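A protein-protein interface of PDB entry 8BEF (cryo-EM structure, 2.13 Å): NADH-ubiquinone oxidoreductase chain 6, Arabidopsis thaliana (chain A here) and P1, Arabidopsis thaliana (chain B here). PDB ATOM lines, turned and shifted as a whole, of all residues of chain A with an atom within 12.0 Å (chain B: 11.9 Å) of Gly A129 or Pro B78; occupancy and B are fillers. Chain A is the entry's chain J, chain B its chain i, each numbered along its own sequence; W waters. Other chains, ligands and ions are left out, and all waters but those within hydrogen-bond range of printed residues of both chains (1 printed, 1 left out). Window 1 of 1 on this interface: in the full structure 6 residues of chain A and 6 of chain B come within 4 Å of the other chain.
Among the printed residues, pairs that only touch across the chains: Ala A128 with Leu B82 (3.8 Å), Ala A128 with Pro B78 (3.8 Å), Gly A129 with Pro B78 (3.8 Å), Trp A134 with Ala B73 (3.8 Å), Ala A128 with Tyr B79 (3.8 Å), Trp A134 with Gly B74 (3.9 Å) and Val A126 with Tyr B79 (3.9 Å).
Val A126 touches just one residue of chain B: Tyr B79.
Of chain B, only Pro B78 comes within 4 Å of Gly A129.
No residue of chain B comes within 4 Å of Val A131.
No residue of chain B comes within 4 Å of Ser A133.
Of the printed residues of chain B, Trp A134 touches Ala B73 (3.8 Å) and Gly B74 (3.9 Å).
Of the printed residues of chain A, Ala B73 touches Trp A134 (3.8 Å).
Printed residues of chain A within 4 Å of Gly B74: Trp A134 (3.9 Å).
Arg B76 touches none of the printed residues of chain A.
Asp B77 touches none of the printed residues of chain A.
Of chain A, only Ala A128 and Gly A129 come within 4 Å of Pro B78.
Tyr B79 touches just these residues of chain A: Val A126 (3.9 Å) and Ala A128 (3.8 Å).
No residue of chain A comes within 4 Å of Asp B80.
Asp B81 touches none of the printed residues of chain A.
Leu B82 touches just one residue of chain A: Ala A128.
The nearest residue of chain A that does not touch Pro B78 is Val A126 (5.2 Å).
The nearest printed residue of chain A that does not touch Gly B74 is Thr A139 (6.1 Å).
Of the 15 printed residues of chain B, 5 touch a printed residue of chain A.
Hydrophobic or aromatic side chains of chain B that line the printed part of chain A: Pro B78, Tyr B79 and Leu B82.
Of the 15 printed residues of chain A, 4 touch a printed residue of chain B.
Among the printed residues, 7 pairs touch across the chains.
Among the printed residues, no Asp or Glu carboxylate lies within 4 Å of a Lys or Arg side-chain nitrogen of the other chain.
Water W1 lies within hydrogen-bond range of N of Ala A128 (2.8 Å), OH of Tyr B79 (3.0 Å) and N of Tyr A127 (3.2 Å).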
ATOM      1  N   TYR A 124      -4.969 -11.677  -8.688  1.00  0.00           N
ATOM      2  CA  TYR A 124      -5.904 -11.624  -7.571  1.00  0.00           C
ATOM      3  C   TYR A 124      -5.719 -12.854  -6.692  1.00  0.00           C
ATOM      4  O   TYR A 124      -5.712 -13.983  -7.189  1.00  0.00           O
ATOM      5  CB  TYR A 124      -7.343 -11.543  -8.083  1.00  0.00           C
ATOM      6  CG  TYR A 124      -8.384 -11.417  -6.994  1.00  0.00           C
ATOM      7  CD1 TYR A 124      -8.273 -10.444  -6.008  1.00  0.00           C
ATOM      8  CD2 TYR A 124      -9.478 -12.272  -6.951  1.00  0.00           C
ATOM      9  CE1 TYR A 124      -9.218 -10.326  -5.016  1.00  0.00           C
ATOM     10  CE2 TYR A 124     -10.428 -12.161  -5.958  1.00  0.00           C
ATOM     11  CZ  TYR A 124     -10.292 -11.188  -4.993  1.00  0.00           C
ATOM     12  OH  TYR A 124     -11.236 -11.076  -4.005  1.00  0.00           O
ATOM     13  N   THR A 125      -5.575 -12.635  -5.388  1.00  0.00           N
ATOM     14  CA  THR A 125      -5.342 -13.706  -4.427  1.00  0.00           C
ATOM     15  C   THR A 125      -6.618 -13.974  -3.639  1.00  0.00           C
ATOM     16  O   THR A 125      -7.182 -13.058  -3.033  1.00  0.00           O
ATOM     17  CB  THR A 125      -4.199 -13.351  -3.476  1.00  0.00           C
ATOM     18  OG1 THR A 125      -2.965 -13.332  -4.203  1.00  0.00           O
ATOM     19  CG2 THR A 125      -4.105 -14.360  -2.348  1.00  0.00           C
ATOM     20  N   VAL A 126      -7.062 -15.226  -3.647  1.00  0.00           N
ATOM     21  CA  VAL A 126      -8.184 -15.684  -2.835  1.00  0.00           C
ATOM     22  C   VAL A 126      -7.604 -16.530  -1.711  1.00  0.00           C
ATOM     23  O   VAL A 126      -7.129 -17.647  -1.945  1.00  0.00           O
ATOM     24  CB  VAL A 126      -9.202 -16.481  -3.661  1.00  0.00           C
ATOM     25  CG1 VAL A 126     -10.403 -16.863  -2.802  1.00  0.00           C
ATOM     26  CG2 VAL A 126      -9.630 -15.691  -4.883  1.00  0.00           C
ATOM     27  N   TYR A 127      -7.640 -16.005  -0.485  1.00  0.00           N
ATOM     28  CA  TYR A 127      -7.055 -16.730   0.633  1.00  0.00           C
ATOM     29  C   TYR A 127      -7.923 -17.899   1.087  1.00  0.00           C
ATOM     30  O   TYR A 127      -7.432 -18.766   1.816  1.00  0.00           O
ATOM     31  CB  TYR A 127      -6.804 -15.789   1.814  1.00  0.00           C
ATOM     32  CG  TYR A 127      -5.783 -14.700   1.581  1.00  0.00           C
ATOM     33  CD1 TYR A 127      -4.429 -14.952   1.725  1.00  0.00           C
ATOM     34  CD2 TYR A 127      -6.178 -13.406   1.255  1.00  0.00           C
ATOM     35  CE1 TYR A 127      -3.492 -13.960   1.523  1.00  0.00           C
ATOM     36  CE2 TYR A 127      -5.248 -12.405   1.053  1.00  0.00           C
ATOM     37  CZ  TYR A 127      -3.903 -12.689   1.191  1.00  0.00           C
ATOM     38  OH  TYR A 127      -2.962 -11.708   0.994  1.00  0.00           O
ATOM     39  N   ALA A 128      -9.190 -17.944   0.668  1.00  0.00           N
ATOM     40  CA  ALA A 128     -10.095 -18.986   1.149  1.00  0.00           C
ATOM     41  C   ALA A 128      -9.601 -20.375   0.762  1.00  0.00           C
ATOM     42  O   ALA A 128      -9.654 -21.310   1.570  1.00  0.00           O
ATOM     43  CB  ALA A 128     -11.505 -18.748   0.614  1.00  0.00           C
ATOM     44  N   GLY A 129      -9.109 -20.531  -0.464  1.00  0.00           N
ATOM     45  CA  GLY A 129      -8.574 -21.810  -0.892  1.00  0.00           C
ATOM     46  C   GLY A 129      -7.225 -22.162  -0.298  1.00  0.00           C
ATOM     47  O   GLY A 129      -6.743 -23.275  -0.529  1.00  0.00           O
ATOM     48  N   LYS A 130      -6.616 -21.254   0.463  1.00  0.00           N
ATOM     49  CA  LYS A 130      -5.288 -21.458   1.028  1.00  0.00           C
ATOM     50  C   LYS A 130      -5.303 -21.849   2.501  1.00  0.00           C
ATOM     51  O   LYS A 130      -4.233 -22.059   3.078  1.00  0.00           O
ATOM     52  CB  LYS A 130      -4.441 -20.192   0.852  1.00  0.00           C
ATOM     53  CG  LYS A 130      -3.858 -20.005  -0.533  1.00  0.00           C
ATOM     54  CD  LYS A 130      -3.324 -18.596  -0.718  1.00  0.00           C
ATOM     55  CE  LYS A 130      -3.172 -18.250  -2.184  1.00  0.00           C
ATOM     56  NZ  LYS A 130      -1.747 -18.221  -2.594  1.00  0.00           N
ATOM     57  N   VAL A 131      -6.480 -21.933   3.125  1.00  0.00           N
ATOM     58  CA  VAL A 131      -6.550 -22.298   4.538  1.00  0.00           C
ATOM     59  C   VAL A 131      -6.087 -23.736   4.738  1.00  0.00           C
ATOM     60  O   VAL A 131      -5.316 -24.035   5.653  1.00  0.00           O
ATOM     61  CB  VAL A 131      -7.981 -22.082   5.071  1.00  0.00           C
ATOM     62  CG1 VAL A 131      -8.172 -22.770   6.415  1.00  0.00           C
ATOM     63  CG2 VAL A 131      -8.315 -20.593   5.156  1.00  0.00           C
ATOM     64  N   ARG A 132      -6.545 -24.641   3.877  1.00  0.00           N
ATOM     65  CA  ARG A 132      -6.203 -26.067   3.907  1.00  0.00           C
ATOM     66  C   ARG A 132      -5.891 -26.507   2.484  1.00  0.00           C
ATOM     67  O   ARG A 132      -6.780 -26.968   1.766  1.00  0.00           O
ATOM     68  CB  ARG A 132      -7.332 -26.896   4.501  1.00  0.00           C
ATOM     69  CG  ARG A 132      -7.038 -28.386   4.587  1.00  0.00           C
ATOM     70  CD  ARG A 132      -8.148 -29.144   5.242  1.00  0.00           C
ATOM     71  NE  ARG A 132      -7.892 -30.573   5.363  1.00  0.00           N
ATOM     72  CZ  ARG A 132      -8.638 -31.405   6.072  1.00  0.00           C
ATOM     73  NH1 ARG A 132      -9.695 -30.976   6.746  1.00  0.00           N
ATOM     74  NH2 ARG A 132      -8.329 -32.698   6.093  1.00  0.00           N
ATOM     75  N   SER A 133      -4.625 -26.395   2.098  1.00  0.00           N
ATOM     76  CA  SER A 133      -4.219 -26.781   0.757  1.00  0.00           C
ATOM     77  C   SER A 133      -4.026 -28.290   0.675  1.00  0.00           C
ATOM     78  O   SER A 133      -3.578 -28.927   1.630  1.00  0.00           O
ATOM     79  CB  SER A 133      -2.931 -26.060   0.355  1.00  0.00           C
ATOM     80  OG  SER A 133      -1.986 -26.086   1.412  1.00  0.00           O
ATOM     81  N   TRP A 134      -4.386 -28.855  -0.470  1.00  0.00           N
ATOM     82  CA  TRP A 134      -4.245 -30.281  -0.727  1.00  0.00           C
ATOM     83  C   TRP A 134      -2.999 -30.537  -1.560  1.00  0.00           C
ATOM     84  O   TRP A 134      -2.728 -29.820  -2.525  1.00  0.00           O
ATOM     85  CB  TRP A 134      -5.468 -30.832  -1.464  1.00  0.00           C
ATOM     86  CG  TRP A 134      -6.628 -31.170  -0.583  1.00  0.00           C
ATOM     87  CD1 TRP A 134      -6.861 -30.716   0.683  1.00  0.00           C
ATOM     88  CD2 TRP A 134      -7.721 -32.041  -0.905  1.00  0.00           C
ATOM     89  NE1 TRP A 134      -8.030 -31.251   1.170  1.00  0.00           N
ATOM     90  CE2 TRP A 134      -8.577 -32.068   0.214  1.00  0.00           C
ATOM     91  CE3 TRP A 134      -8.055 -32.803  -2.028  1.00  0.00           C
ATOM     92  CZ2 TRP A 134      -9.749 -32.824   0.239  1.00  0.00           C
ATOM     93  CZ3 TRP A 134      -9.218 -33.553  -2.001  1.00  0.00           C
ATOM     94  CH2 TRP A 134     -10.051 -33.555  -0.877  1.00  0.00           C
ATOM     95  N   THR A 135      -2.248 -31.570  -1.191  1.00  0.00           N
ATOM     96  CA  THR A 135      -1.169 -32.025  -2.052  1.00  0.00           C
ATOM     97  C   THR A 135      -1.737 -32.694  -3.305  1.00  0.00           C
ATOM     98  O   THR A 135      -2.893 -33.122  -3.345  1.00  0.00           O
ATOM     99  CB  THR A 135      -0.247 -32.995  -1.308  1.00  0.00           C
ATOM    100  OG1 THR A 135      -0.913 -34.249  -1.117  1.00  0.00           O
ATOM    101  CG2 THR A 135       0.154 -32.423   0.048  1.00  0.00           C
ATOM    102  N   ASN A 136      -0.903 -32.755  -4.346  1.00  0.00           N
ATOM    103  CA  ASN A 136      -1.235 -33.534  -5.536  1.00  0.00           C
ATOM    104  C   ASN A 136      -1.612 -34.963  -5.154  1.00  0.00           C
ATOM    105  O   ASN A 136      -2.594 -35.522  -5.665  1.00  0.00           O
ATOM    106  CB  ASN A 136      -0.037 -33.508  -6.495  1.00  0.00           C
ATOM    107  CG  ASN A 136      -0.279 -34.275  -7.784  1.00  0.00           C
ATOM    108  OD1 ASN A 136       0.664 -34.762  -8.404  1.00  0.00           O
ATOM    109  ND2 ASN A 136      -1.535 -34.372  -8.202  1.00  0.00           N
ATOM    110  N   GLU A 138      -2.898 -36.238  -2.267  1.00  0.00           N
ATOM    111  CA  GLU A 138      -4.196 -36.436  -1.636  1.00  0.00           C
ATOM    112  C   GLU A 138      -5.354 -36.042  -2.548  1.00  0.00           C
ATOM    113  O   GLU A 138      -6.426 -36.650  -2.462  1.00  0.00           O
ATOM    114  CB  GLU A 138      -4.252 -35.706  -0.292  1.00  0.00           C
ATOM    115  CG  GLU A 138      -4.075 -34.214  -0.314  1.00  0.00           C
ATOM    116  CD  GLU A 138      -3.332 -33.722   0.925  1.00  0.00           C
ATOM    117  OE1 GLU A 138      -2.994 -34.556   1.787  1.00  0.00           O
ATOM    118  OE2 GLU A 138      -3.081 -32.509   1.039  1.00  0.00           O
ATOM    119  N   THR A 139      -5.151 -35.087  -3.460  1.00  0.00           N
ATOM    120  CA  THR A 139      -6.183 -34.805  -4.456  1.00  0.00           C
ATOM    121  C   THR A 139      -6.424 -36.011  -5.358  1.00  0.00           C
ATOM    122  O   THR A 139      -7.574 -36.338  -5.669  1.00  0.00           O
ATOM    123  CB  THR A 139      -5.811 -33.573  -5.286  1.00  0.00           C
ATOM    124  OG1 THR A 139      -5.393 -32.510  -4.420  1.00  0.00           O
ATOM    125  CG2 THR A 139      -7.004 -33.106  -6.116  1.00  0.00           C
ATOM    126  N   SER B  70     -22.405 -32.325  -4.342  1.00  0.00           N
ATOM    127  CA  SER B  70     -21.949 -30.940  -4.360  1.00  0.00           C
ATOM    128  C   SER B  70     -21.286 -30.516  -3.054  1.00  0.00           C
ATOM    129  O   SER B  70     -20.574 -29.509  -3.038  1.00  0.00           O
ATOM    130  CB  SER B  70     -23.123 -30.009  -4.680  1.00  0.00           C
ATOM    131  OG  SER B  70     -24.049 -29.972  -3.613  1.00  0.00           O
ATOM    132  N   GLN B  71     -21.500 -31.253  -1.968  1.00  0.00           N
ATOM    133  CA  GLN B  71     -20.896 -30.950  -0.679  1.00  0.00           C
ATOM    134  C   GLN B  71     -19.691 -31.833  -0.376  1.00  0.00           C
ATOM    135  O   GLN B  71     -19.212 -31.841   0.760  1.00  0.00           O
ATOM    136  CB  GLN B  71     -21.939 -31.084   0.434  1.00  0.00           C
ATOM    137  CG  GLN B  71     -22.723 -29.813   0.721  1.00  0.00           C
ATOM    138  CD  GLN B  71     -22.877 -28.929  -0.499  1.00  0.00           C
ATOM    139  OE1 GLN B  71     -23.614 -29.253  -1.428  1.00  0.00           O
ATOM    140  NE2 GLN B  71     -22.173 -27.806  -0.504  1.00  0.00           N
ATOM    141  N   VAL B  72     -19.197 -32.574  -1.362  1.00  0.00           N
ATOM    142  CA  VAL B  72     -18.111 -33.523  -1.145  1.00  0.00           C
ATOM    143  C   VAL B  72     -16.778 -32.788  -1.194  1.00  0.00           C
ATOM    144  O   VAL B  72     -16.530 -31.984  -2.100  1.00  0.00           O
ATOM    145  CB  VAL B  72     -18.166 -34.651  -2.187  1.00  0.00           C
ATOM    146  CG1 VAL B  72     -16.876 -35.455  -2.181  1.00  0.00           C
ATOM    147  CG2 VAL B  72     -19.370 -35.547  -1.933  1.00  0.00           C
ATOM    148  N   ALA B  73     -15.917 -33.064  -0.216  1.00  0.00           N
ATOM    149  CA  ALA B  73     -14.593 -32.458  -0.187  1.00  0.00           C
ATOM    150  C   ALA B  73     -13.821 -32.813  -1.453  1.00  0.00           C
ATOM    151  O   ALA B  73     -13.736 -33.981  -1.840  1.00  0.00           O
ATOM    152  CB  ALA B  73     -13.828 -32.917   1.053  1.00  0.00           C
ATOM    153  N   GLY B  74     -13.261 -31.793  -2.095  1.00  0.00           N
ATOM    154  CA  GLY B  74     -12.607 -31.924  -3.377  1.00  0.00           C
ATOM    155  C   GLY B  74     -13.299 -31.187  -4.504  1.00  0.00           C
ATOM    156  O   GLY B  74     -12.676 -30.956  -5.546  1.00  0.00           O
ATOM    157  N   ARG B  75     -14.569 -30.802  -4.326  1.00  0.00           N
ATOM    158  CA  ARG B  75     -15.279 -30.073  -5.371  1.00  0.00           C
ATOM    159  C   ARG B  75     -16.146 -28.948  -4.811  1.00  0.00           C
ATOM    160  O   ARG B  75     -17.027 -28.448  -5.518  1.00  0.00           O
ATOM    161  CB  ARG B  75     -16.138 -31.028  -6.214  1.00  0.00           C
ATOM    162  CG  ARG B  75     -17.225 -31.750  -5.439  1.00  0.00           C
ATOM    163  CD  ARG B  75     -17.803 -32.903  -6.243  1.00  0.00           C
ATOM    164  NE  ARG B  75     -18.613 -32.447  -7.366  1.00  0.00           N
ATOM    165  CZ  ARG B  75     -18.244 -32.521  -8.636  1.00  0.00           C
ATOM    166  NH1 ARG B  75     -17.071 -33.026  -8.987  1.00  0.00           N
ATOM    167  NH2 ARG B  75     -19.069 -32.078  -9.578  1.00  0.00           N
ATOM    168  N   ARG B  76     -15.914 -28.530  -3.573  1.00  0.00           N
ATOM    169  CA  ARG B  76     -16.691 -27.471  -2.951  1.00  0.00           C
ATOM    170  C   ARG B  76     -16.110 -26.100  -3.271  1.00  0.00           C
ATOM    171  O   ARG B  76     -14.902 -25.944  -3.466  1.00  0.00           O
ATOM    172  CB  ARG B  76     -16.737 -27.665  -1.437  1.00  0.00           C
ATOM    173  CG  ARG B  76     -17.104 -29.069  -1.025  1.00  0.00           C
ATOM    174  CD  ARG B  76     -17.404 -29.150   0.446  1.00  0.00           C
ATOM    175  NE  ARG B  76     -18.611 -28.412   0.793  1.00  0.00           N
ATOM    176  CZ  ARG B  76     -18.927 -28.040   2.025  1.00  0.00           C
ATOM    177  NH1 ARG B  76     -18.152 -28.334   3.053  1.00  0.00           N
ATOM    178  NH2 ARG B  76     -20.048 -27.356   2.227  1.00  0.00           N
ATOM    179  N   ASP B  77     -16.990 -25.108  -3.333  1.00  0.00           N
ATOM    180  CA  ASP B  77     -16.546 -23.723  -3.349  1.00  0.00           C
ATOM    181  C   ASP B  77     -15.784 -23.447  -2.056  1.00  0.00           C
ATOM    182  O   ASP B  77     -16.250 -23.837  -0.977  1.00  0.00           O
ATOM    183  CB  ASP B  77     -17.747 -22.780  -3.489  1.00  0.00           C
ATOM    184  CG  ASP B  77     -17.351 -21.308  -3.611  1.00  0.00           C
ATOM    185  OD1 ASP B  77     -16.147 -20.985  -3.610  1.00  0.00           O
ATOM    186  OD2 ASP B  77     -18.254 -20.459  -3.728  1.00  0.00           O
ATOM    187  N   PRO B  78     -14.616 -22.802  -2.116  1.00  0.00           N
ATOM    188  CA  PRO B  78     -13.834 -22.591  -0.886  1.00  0.00           C
ATOM    189  C   PRO B  78     -14.576 -21.825   0.197  1.00  0.00           C
ATOM    190  O   PRO B  78     -14.295 -22.033   1.383  1.00  0.00           O
ATOM    191  CB  PRO B  78     -12.598 -21.822  -1.381  1.00  0.00           C
ATOM    192  CG  PRO B  78     -12.928 -21.369  -2.770  1.00  0.00           C
ATOM    193  CD  PRO B  78     -13.871 -22.387  -3.314  1.00  0.00           C
ATOM    194  N   TYR B  79     -15.526 -20.962  -0.165  1.00  0.00           N
ATOM    195  CA  TYR B  79     -16.245 -20.194   0.844  1.00  0.00           C
ATOM    196  C   TYR B  79     -17.262 -21.028   1.620  1.00  0.00           C
ATOM    197  O   TYR B  79     -17.710 -20.593   2.683  1.00  0.00           O
ATOM    198  CB  TYR B  79     -16.929 -18.994   0.193  1.00  0.00           C
ATOM    199  CG  TYR B  79     -15.955 -17.893  -0.150  1.00  0.00           C
ATOM    200  CD1 TYR B  79     -15.285 -17.204   0.852  1.00  0.00           C
ATOM    201  CD2 TYR B  79     -15.684 -17.562  -1.471  1.00  0.00           C
ATOM    202  CE1 TYR B  79     -14.385 -16.206   0.550  1.00  0.00           C
ATOM    203  CE2 TYR B  79     -14.783 -16.566  -1.781  1.00  0.00           C
ATOM    204  CZ  TYR B  79     -14.138 -15.891  -0.766  1.00  0.00           C
ATOM    205  OH  TYR B  79     -13.241 -14.896  -1.064  1.00  0.00           O
ATOM    206  N   ASP B  80     -17.636 -22.209   1.118  1.00  0.00           N
ATOM    207  CA  ASP B  80     -18.570 -23.064   1.849  1.00  0.00           C
ATOM    208  C   ASP B  80     -17.992 -23.534   3.177  1.00  0.00           C
ATOM    209  O   ASP B  80     -18.731 -23.686   4.155  1.00  0.00           O
ATOM    210  CB  ASP B  80     -18.966 -24.269   0.997  1.00  0.00           C
ATOM    211  CG  ASP B  80     -19.260 -23.894  -0.433  1.00  0.00           C
ATOM    212  OD1 ASP B  80     -19.514 -22.702  -0.683  1.00  0.00           O
ATOM    213  OD2 ASP B  80     -19.227 -24.784  -1.306  1.00  0.00           O
ATOM    214  N   ASP B  81     -16.683 -23.777   3.232  1.00  0.00           N
ATOM    215  CA  ASP B  81     -16.070 -24.212   4.480  1.00  0.00           C
ATOM    216  C   ASP B  81     -16.025 -23.078   5.499  1.00  0.00           C
ATOM    217  O   ASP B  81     -16.183 -23.313   6.702  1.00  0.00           O
ATOM    218  CB  ASP B  81     -14.670 -24.759   4.211  1.00  0.00           C
ATOM    219  CG  ASP B  81     -14.417 -26.077   4.913  1.00  0.00           C
ATOM    220  OD1 ASP B  81     -15.213 -26.438   5.806  1.00  0.00           O
ATOM    221  OD2 ASP B  81     -13.422 -26.751   4.576  1.00  0.00           O
ATOM    222  N   LEU B  82     -15.810 -21.842   5.039  1.00  0.00           N
ATOM    223  CA  LEU B  82     -15.755 -20.703   5.948  1.00  0.00           C
ATOM    224  C   LEU B  82     -17.094 -20.420   6.614  1.00  0.00           C
ATOM    225  O   LEU B  82     -17.117 -19.913   7.739  1.00  0.00           O
ATOM    226  CB  LEU B  82     -15.289 -19.445   5.211  1.00  0.00           C
ATOM    227  CG  LEU B  82     -13.800 -19.277   4.904  1.00  0.00           C
ATOM    228  CD1 LEU B  82     -12.971 -19.707   6.092  1.00  0.00           C
ATOM    229  CD2 LEU B  82     -13.389 -20.038   3.666  1.00  0.00           C
ATOM    230  N   LEU B  83     -18.202 -20.728   5.947  1.00  0.00           N
ATOM    231  CA  LEU B  83     -19.523 -20.428   6.478  1.00  0.00           C
ATOM    232  C   LEU B  83     -20.216 -21.637   7.087  1.00  0.00           C
ATOM    233  O   LEU B  83     -21.265 -21.471   7.718  1.00  0.00           O
ATOM    234  CB  LEU B  83     -20.402 -19.828   5.378  1.00  0.00           C
ATOM    235  CG  LEU B  83     -20.102 -18.350   5.128  1.00  0.00           C
ATOM    236  CD1 LEU B  83     -21.061 -17.749   4.118  1.00  0.00           C
ATOM    237  CD2 LEU B  83     -20.151 -17.584   6.435  1.00  0.00           C
ATOM    238  N   GLU B  84     -19.662 -22.834   6.929  1.00  0.00           N
ATOM    239  CA  GLU B  84     -20.258 -24.031   7.510  1.00  0.00           C
ATOM    240  C   GLU B  84     -19.382 -24.586   8.628  1.00  0.00           C
ATOM    241  O   GLU B  84     -19.883 -25.175   9.588  1.00  0.00           O
ATOM    242  CB  GLU B  84     -20.480 -25.098   6.435  1.00  0.00           C
ATOM    243  CG  GLU B  84     -21.797 -24.963   5.686  1.00  0.00           C
ATOM    244  CD  GLU B  84     -22.989 -25.404   6.512  1.00  0.00           C
ATOM    245  OE1 GLU B  84     -22.841 -26.351   7.314  1.00  0.00           O
ATOM    246  OE2 GLU B  84     -24.074 -24.805   6.358  1.00  0.00           O
HETATM  247  O   HOH W   1     -10.681 -15.566   0.290  1.00  0.00           O
